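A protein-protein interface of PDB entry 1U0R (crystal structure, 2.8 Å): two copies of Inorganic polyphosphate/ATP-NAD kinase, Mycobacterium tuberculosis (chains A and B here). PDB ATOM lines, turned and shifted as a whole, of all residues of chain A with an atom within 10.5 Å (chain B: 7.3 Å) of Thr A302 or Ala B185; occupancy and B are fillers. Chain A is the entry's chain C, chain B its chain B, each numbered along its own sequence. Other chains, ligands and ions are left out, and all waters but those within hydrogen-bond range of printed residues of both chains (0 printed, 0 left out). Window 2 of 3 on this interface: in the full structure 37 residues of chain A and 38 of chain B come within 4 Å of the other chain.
The backbone carbonyl oxygen (O) of Pro A300 lies within hydrogen-bond range of the backbone NH (N) of Ala B185.
The backbone NH (N) of Val B183 lies within hydrogen-bond range of the backbone carbonyl oxygen (O) of Val B176 (2.9 Å).
O of Ser B184 lies within hydrogen-bond range of N of Val B176, 2.9 Å away.
N of Leu A299 is in hydrogen-bond range of O of Val A294, 3.1 Å away.
Among the printed residues, merely in contact across the chains: Thr A290 with Pro B182 (3.2 Å), Val A294 with Pro B182 (3.6 Å), Leu A299 with Val B183 (3.6 Å), Pro A300 with Ser B184 (3.5 Å), Val A301 with Pro B182 (3.2 Å), Val A301 with Val B183 (3.9 Å), Val A301 with Ser B184 (3.8 Å), Thr A302 with Ala B185 (3.4 Å), Trp A304 with Val B175 (3.7 Å) and Trp A304 with Pro B182 (3.6 Å).
Of the printed residues of chain B, Leu A299 touches Val B183 (3.6 Å).
Thr A302 touches one residue of chain B.
Printed residues of chain B within 4 Å of Trp A304: Val B175 (3.7 Å) and Pro B182 (3.6 Å).
Printed residues of chain A within 4 Å of Val B175: Trp A304.
Printed residues of chain A within 4 Å of Pro B182: Thr A290, Val A294, Val A301 and Trp A304.
Of the printed residues of chain A, Val B183 touches Leu A299 and Val A301.
Of chain A, only Pro A300 and Val A301 come within 4 Å of Ser B184.
Ala B185 touches just these residues of chain A: Pro A300 and Thr A302.
No residue of chain A comes within 4 Å of Phe B186.
The nearest residue of chain B that does not touch Thr A302 is Val B175 (4.3 Å).
The nearest residue of chain A that does not touch Ala B185 is Val A301 (4.2 Å).
The nearest printed residue of chain A that does not touch Val B175 is Gly A303 (4.2 Å).
Printed residues of chain A that touch a printed residue of chain B: Thr A290, Val A294, Leu A299, Pro A300, Val A301, Thr A302 and Trp A304.
Hydrophobic or aromatic side chains of chain A within 4 Å of the printed part of chain B: Val A294, Leu A299, Val A301 and Trp A304.
No position is printed for both chains.
Of the 11 pairs that touch across the chains among the printed residues, none has its exchanged pair printed and touching as well.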
ATOM      1  N   THR A 290      28.590 -18.781  19.037  1.00  0.00           N
ATOM      2  CA  THR A 290      28.348 -17.374  19.213  1.00  0.00           C
ATOM      3  C   THR A 290      29.318 -16.831  20.226  1.00  0.00           C
ATOM      4  O   THR A 290      30.077 -15.949  19.908  1.00  0.00           O
ATOM      5  CB  THR A 290      26.914 -17.141  19.656  1.00  0.00           C
ATOM      6  OG1 THR A 290      26.023 -17.540  18.610  1.00  0.00           O
ATOM      7  CG2 THR A 290      26.644 -15.692  19.807  1.00  0.00           C
ATOM      8  N   VAL A 294      32.259 -13.885  19.714  1.00  0.00           N
ATOM      9  CA  VAL A 294      32.271 -12.656  20.455  1.00  0.00           C
ATOM     10  C   VAL A 294      33.597 -12.434  21.171  1.00  0.00           C
ATOM     11  O   VAL A 294      34.166 -11.363  21.102  1.00  0.00           O
ATOM     12  CB  VAL A 294      31.104 -12.640  21.431  1.00  0.00           C
ATOM     13  CG1 VAL A 294      30.980 -11.291  22.100  1.00  0.00           C
ATOM     14  CG2 VAL A 294      29.841 -12.973  20.695  1.00  0.00           C
ATOM     15  N   ARG A 298      36.122  -9.548  20.012  1.00  0.00           N
ATOM     16  CA  ARG A 298      35.761  -8.484  20.951  1.00  0.00           C
ATOM     17  C   ARG A 298      34.446  -7.773  20.553  1.00  0.00           C
ATOM     18  O   ARG A 298      34.272  -6.569  20.720  1.00  0.00           O
ATOM     19  CB  ARG A 298      36.929  -7.492  21.123  1.00  0.00           C
ATOM     20  CG  ARG A 298      38.285  -8.137  21.439  1.00  0.00           C
ATOM     21  CD  ARG A 298      38.452  -8.618  22.913  1.00  0.00           C
ATOM     22  NE  ARG A 298      39.869  -8.683  23.320  1.00  0.00           N
ATOM     23  CZ  ARG A 298      40.582  -7.657  23.832  1.00  0.00           C
ATOM     24  NH1 ARG A 298      40.021  -6.453  24.036  1.00  0.00           N
ATOM     25  NH2 ARG A 298      41.864  -7.837  24.155  1.00  0.00           N
ATOM     26  N   LEU A 299      33.524  -8.573  20.039  1.00  0.00           N
ATOM     27  CA  LEU A 299      32.261  -8.116  19.456  1.00  0.00           C
ATOM     28  C   LEU A 299      31.419  -7.382  20.476  1.00  0.00           C
ATOM     29  O   LEU A 299      31.229  -7.897  21.560  1.00  0.00           O
ATOM     30  CB  LEU A 299      31.490  -9.335  18.934  1.00  0.00           C
ATOM     31  CG  LEU A 299      31.495  -9.575  17.433  1.00  0.00           C
ATOM     32  CD1 LEU A 299      32.694  -8.984  16.756  1.00  0.00           C
ATOM     33  CD2 LEU A 299      31.357 -11.030  17.120  1.00  0.00           C
ATOM     34  N   PRO A 300      30.901  -6.205  20.142  1.00  0.00           N
ATOM     35  CA  PRO A 300      30.202  -5.378  21.130  1.00  0.00           C
ATOM     36  C   PRO A 300      28.795  -5.897  21.371  1.00  0.00           C
ATOM     37  O   PRO A 300      27.969  -5.965  20.477  1.00  0.00           O
ATOM     38  CB  PRO A 300      30.182  -4.006  20.473  1.00  0.00           C
ATOM     39  CG  PRO A 300      31.071  -4.159  19.280  1.00  0.00           C
ATOM     40  CD  PRO A 300      30.907  -5.563  18.820  1.00  0.00           C
ATOM     41  N   VAL A 301      28.522  -6.288  22.597  1.00  0.00           N
ATOM     42  CA  VAL A 301      27.297  -7.010  22.876  1.00  0.00           C
ATOM     43  C   VAL A 301      26.464  -6.494  24.090  1.00  0.00           C
ATOM     44  O   VAL A 301      25.466  -7.089  24.465  1.00  0.00           O
ATOM     45  CB  VAL A 301      27.654  -8.482  22.930  1.00  0.00           C
ATOM     46  CG1 VAL A 301      27.880  -8.953  24.331  1.00  0.00           C
ATOM     47  CG2 VAL A 301      26.633  -9.280  22.200  1.00  0.00           C
ATOM     48  N   THR A 302      26.862  -5.365  24.675  1.00  0.00           N
ATOM     49  CA  THR A 302      26.098  -4.691  25.730  1.00  0.00           C
ATOM     50  C   THR A 302      24.692  -4.414  25.268  1.00  0.00           C
ATOM     51  O   THR A 302      24.482  -4.176  24.080  1.00  0.00           O
ATOM     52  CB  THR A 302      26.700  -3.323  26.050  1.00  0.00           C
ATOM     53  OG1 THR A 302      26.625  -2.519  24.872  1.00  0.00           O
ATOM     54  CG2 THR A 302      28.238  -3.402  26.381  1.00  0.00           C
ATOM     55  N   GLY A 303      23.745  -4.436  26.207  1.00  0.00           N
ATOM     56  CA  GLY A 303      22.372  -4.048  25.946  1.00  0.00           C
ATOM     57  C   GLY A 303      21.422  -5.198  25.784  1.00  0.00           C
ATOM     58  O   GLY A 303      20.227  -5.014  25.721  1.00  0.00           O
ATOM     59  N   TRP A 304      21.954  -6.398  25.716  1.00  0.00           N
ATOM     60  CA  TRP A 304      21.184  -7.611  25.467  1.00  0.00           C
ATOM     61  C   TRP A 304      20.137  -7.900  26.526  1.00  0.00           C
ATOM     62  O   TRP A 304      20.421  -7.791  27.701  1.00  0.00           O
ATOM     63  CB  TRP A 304      22.175  -8.799  25.391  1.00  0.00           C
ATOM     64  CG  TRP A 304      21.558 -10.125  25.080  1.00  0.00           C
ATOM     65  CD1 TRP A 304      20.658 -10.388  24.102  1.00  0.00           C
ATOM     66  CD2 TRP A 304      21.812 -11.365  25.735  1.00  0.00           C
ATOM     67  NE1 TRP A 304      20.322 -11.719  24.104  1.00  0.00           N
ATOM     68  CE2 TRP A 304      21.013 -12.345  25.108  1.00  0.00           C
ATOM     69  CE3 TRP A 304      22.629 -11.754  26.800  1.00  0.00           C
ATOM     70  CZ2 TRP A 304      20.999 -13.695  25.515  1.00  0.00           C
ATOM     71  CZ3 TRP A 304      22.623 -13.087  27.198  1.00  0.00           C
ATOM     72  CH2 TRP A 304      21.813 -14.042  26.550  1.00  0.00           C
ATOM     73  N   ARG A 305      18.922  -8.232  26.083  1.00  0.00           N
ATOM     74  CA  ARG A 305      17.939  -9.036  26.833  1.00  0.00           C
ATOM     75  C   ARG A 305      18.307  -9.254  28.282  1.00  0.00           C
ATOM     76  O   ARG A 305      19.210 -10.057  28.577  1.00  0.00           O
ATOM     77  CB  ARG A 305      17.879 -10.415  26.199  1.00  0.00           C
ATOM     78  CG  ARG A 305      17.212 -11.479  26.991  1.00  0.00           C
ATOM     79  CD  ARG A 305      16.236 -12.253  26.124  1.00  0.00           C
ATOM     80  NE  ARG A 305      15.939 -13.606  26.597  1.00  0.00           N
ATOM     81  CZ  ARG A 305      14.896 -14.318  26.185  1.00  0.00           C
ATOM     82  NH1 ARG A 305      14.041 -13.801  25.311  1.00  0.00           N
ATOM     83  NH2 ARG A 305      14.693 -15.541  26.659  1.00  0.00           N
ATOM     84  N   GLY B 173      18.762   0.932  17.060  1.00  0.00           N
ATOM     85  CA  GLY B 173      19.546   0.120  17.963  1.00  0.00           C
ATOM     86  C   GLY B 173      18.914  -1.233  17.901  1.00  0.00           C
ATOM     87  O   GLY B 173      17.712  -1.355  17.825  1.00  0.00           O
ATOM     88  N   VAL B 174      19.738  -2.262  17.921  1.00  0.00           N
ATOM     89  CA  VAL B 174      19.305  -3.629  17.682  1.00  0.00           C
ATOM     90  C   VAL B 174      20.371  -4.441  18.326  1.00  0.00           C
ATOM     91  O   VAL B 174      21.557  -4.078  18.252  1.00  0.00           O
ATOM     92  CB  VAL B 174      19.374  -3.913  16.210  1.00  0.00           C
ATOM     93  CG1 VAL B 174      20.077  -5.187  15.964  1.00  0.00           C
ATOM     94  CG2 VAL B 174      17.980  -3.888  15.580  1.00  0.00           C
ATOM     95  N   VAL B 175      19.952  -5.505  19.011  1.00  0.00           N
ATOM     96  CA  VAL B 175      20.841  -6.588  19.436  1.00  0.00           C
ATOM     97  C   VAL B 175      20.438  -7.839  18.654  1.00  0.00           C
ATOM     98  O   VAL B 175      19.292  -8.277  18.703  1.00  0.00           O
ATOM     99  CB  VAL B 175      20.716  -6.812  20.908  1.00  0.00           C
ATOM    100  CG1 VAL B 175      21.471  -8.051  21.318  1.00  0.00           C
ATOM    101  CG2 VAL B 175      21.288  -5.638  21.633  1.00  0.00           C
ATOM    102  N   VAL B 176      21.373  -8.376  17.879  1.00  0.00           N
ATOM    103  CA  VAL B 176      21.138  -9.597  17.105  1.00  0.00           C
ATOM    104  C   VAL B 176      21.630 -10.757  17.942  1.00  0.00           C
ATOM    105  O   VAL B 176      22.684 -10.664  18.589  1.00  0.00           O
ATOM    106  CB  VAL B 176      21.801  -9.590  15.708  1.00  0.00           C
ATOM    107  CG1 VAL B 176      21.486 -10.848  14.981  1.00  0.00           C
ATOM    108  CG2 VAL B 176      21.286  -8.452  14.892  1.00  0.00           C
ATOM    109  N   PRO B 182      23.814 -13.493  22.345  1.00  0.00           N
ATOM    110  CA  PRO B 182      23.983 -12.278  21.569  1.00  0.00           C
ATOM    111  C   PRO B 182      25.268 -12.302  20.717  1.00  0.00           C
ATOM    112  O   PRO B 182      26.316 -12.794  21.152  1.00  0.00           O
ATOM    113  CB  PRO B 182      24.112 -11.224  22.669  1.00  0.00           C
ATOM    114  CG  PRO B 182      24.793 -11.913  23.725  1.00  0.00           C
ATOM    115  CD  PRO B 182      24.171 -13.278  23.757  1.00  0.00           C
ATOM    116  N   VAL B 183      25.214 -11.723  19.527  1.00  0.00           N
ATOM    117  CA  VAL B 183      26.385 -11.688  18.671  1.00  0.00           C
ATOM    118  C   VAL B 183      26.824 -10.263  18.415  1.00  0.00           C
ATOM    119  O   VAL B 183      28.012 -10.017  18.165  1.00  0.00           O
ATOM    120  CB  VAL B 183      26.185 -12.517  17.362  1.00  0.00           C
ATOM    121  CG1 VAL B 183      25.144 -11.936  16.484  1.00  0.00           C
ATOM    122  CG2 VAL B 183      27.403 -12.557  16.595  1.00  0.00           C
ATOM    123  N   SER B 184      25.893  -9.307  18.461  1.00  0.00           N
ATOM    124  CA  SER B 184      26.232  -7.924  18.112  1.00  0.00           C
ATOM    125  C   SER B 184      25.157  -6.962  18.435  1.00  0.00           C
ATOM    126  O   SER B 184      23.985  -7.231  18.229  1.00  0.00           O
ATOM    127  CB  SER B 184      26.518  -7.778  16.638  1.00  0.00           C
ATOM    128  OG  SER B 184      27.910  -7.878  16.432  1.00  0.00           O
ATOM    129  N   ALA B 185      25.596  -5.819  18.930  1.00  0.00           N
ATOM    130  CA  ALA B 185      24.761  -4.700  19.248  1.00  0.00           C
ATOM    131  C   ALA B 185      25.346  -3.646  18.362  1.00  0.00           C
ATOM    132  O   ALA B 185      26.543  -3.530  18.318  1.00  0.00           O
ATOM    133  CB  ALA B 185      24.966  -4.324  20.693  1.00  0.00           C
ATOM    134  N   PHE B 186      24.516  -2.900  17.645  1.00  0.00           N
ATOM    135  CA  PHE B 186      24.967  -1.809  16.792  1.00  0.00           C
ATOM    136  C   PHE B 186      23.768  -1.058  16.297  1.00  0.00           C
ATOM    137  O   PHE B 186      22.656  -1.535  16.446  1.00  0.00           O
ATOM    138  CB  PHE B 186      25.785  -2.332  15.595  1.00  0.00           C
ATOM    139  CG  PHE B 186      25.095  -3.425  14.792  1.00  0.00           C
ATOM    140  CD1 PHE B 186      23.947  -3.164  14.059  1.00  0.00           C
ATOM    141  CD2 PHE B 186      25.625  -4.702  14.755  1.00  0.00           C
ATOM    142  CE1 PHE B 186      23.348  -4.148  13.357  1.00  0.00           C
ATOM    143  CE2 PHE B 186      25.020  -5.680  14.048  1.00  0.00           C
ATOM    144  CZ  PHE B 186      23.889  -5.414  13.350  1.00  0.00           C
ATOM    145  N   GLY B 187      23.976   0.108  15.697  1.00  0.00           N
ATOM    146  CA  GLY B 187      22.862   0.849  15.142  1.00  0.00           C
ATOM    147  C   GLY B 187      22.944   0.567  13.672  1.00  0.00           C
ATOM    148  O   GLY B 187      24.046   0.277  13.205  1.00  0.00           O
ATOM    149  N   HIS B 226      26.317   0.558  11.489  1.00  0.00           N
ATOM    150  CA  HIS B 226      27.472   1.376  11.792  1.00  0.00           C
ATOM    151  C   HIS B 226      28.369   0.637  12.777  1.00  0.00           C
ATOM    152  O   HIS B 226      28.310   0.894  13.970  1.00  0.00           O
ATOM    153  CB  HIS B 226      27.045   2.692  12.400  1.00  0.00           C
ATOM    154  CG  HIS B 226      28.067   3.756  12.260  1.00  0.00           C
ATOM    155  ND1 HIS B 226      28.734   4.285  13.336  1.00  0.00           N
ATOM    156  CD2 HIS B 226      28.556   4.391  11.168  1.00  0.00           C
ATOM    157  CE1 HIS B 226      29.584   5.212  12.923  1.00  0.00           C
ATOM    158  NE2 HIS B 226      29.495   5.299  11.610  1.00  0.00           N
ATOM    159  N   ALA B 227      29.219  -0.252  12.302  1.00  0.00           N
ATOM    160  CA  ALA B 227      29.941  -1.098  13.214  1.00  0.00           C
ATOM    161  C   ALA B 227      30.987  -1.861  12.484  1.00  0.00           C
ATOM    162  O   ALA B 227      31.032  -1.902  11.258  1.00  0.00           O
ATOM    163  CB  ALA B 227      29.020  -2.039  13.850  1.00  0.00           C
ATOM    164  N   PHE B 229      31.978  -5.003  12.423  1.00  0.00           N
ATOM    165  CA  PHE B 229      31.611  -6.298  11.924  1.00  0.00           C
ATOM    166  C   PHE B 229      30.159  -6.140  11.602  1.00  0.00           C
ATOM    167  O   PHE B 229      29.342  -5.965  12.508  1.00  0.00           O
ATOM    168  CB  PHE B 229      31.789  -7.269  13.057  1.00  0.00           C
ATOM    169  CG  PHE B 229      31.119  -8.589  12.867  1.00  0.00           C
ATOM    170  CD1 PHE B 229      31.701  -9.579  12.103  1.00  0.00           C
ATOM    171  CD2 PHE B 229      29.954  -8.882  13.524  1.00  0.00           C
ATOM    172  CE1 PHE B 229      31.091 -10.811  11.988  1.00  0.00           C
ATOM    173  CE2 PHE B 229      29.361 -10.105  13.386  1.00  0.00           C
ATOM    174  CZ  PHE B 229      29.935 -11.060  12.630  1.00  0.00           C
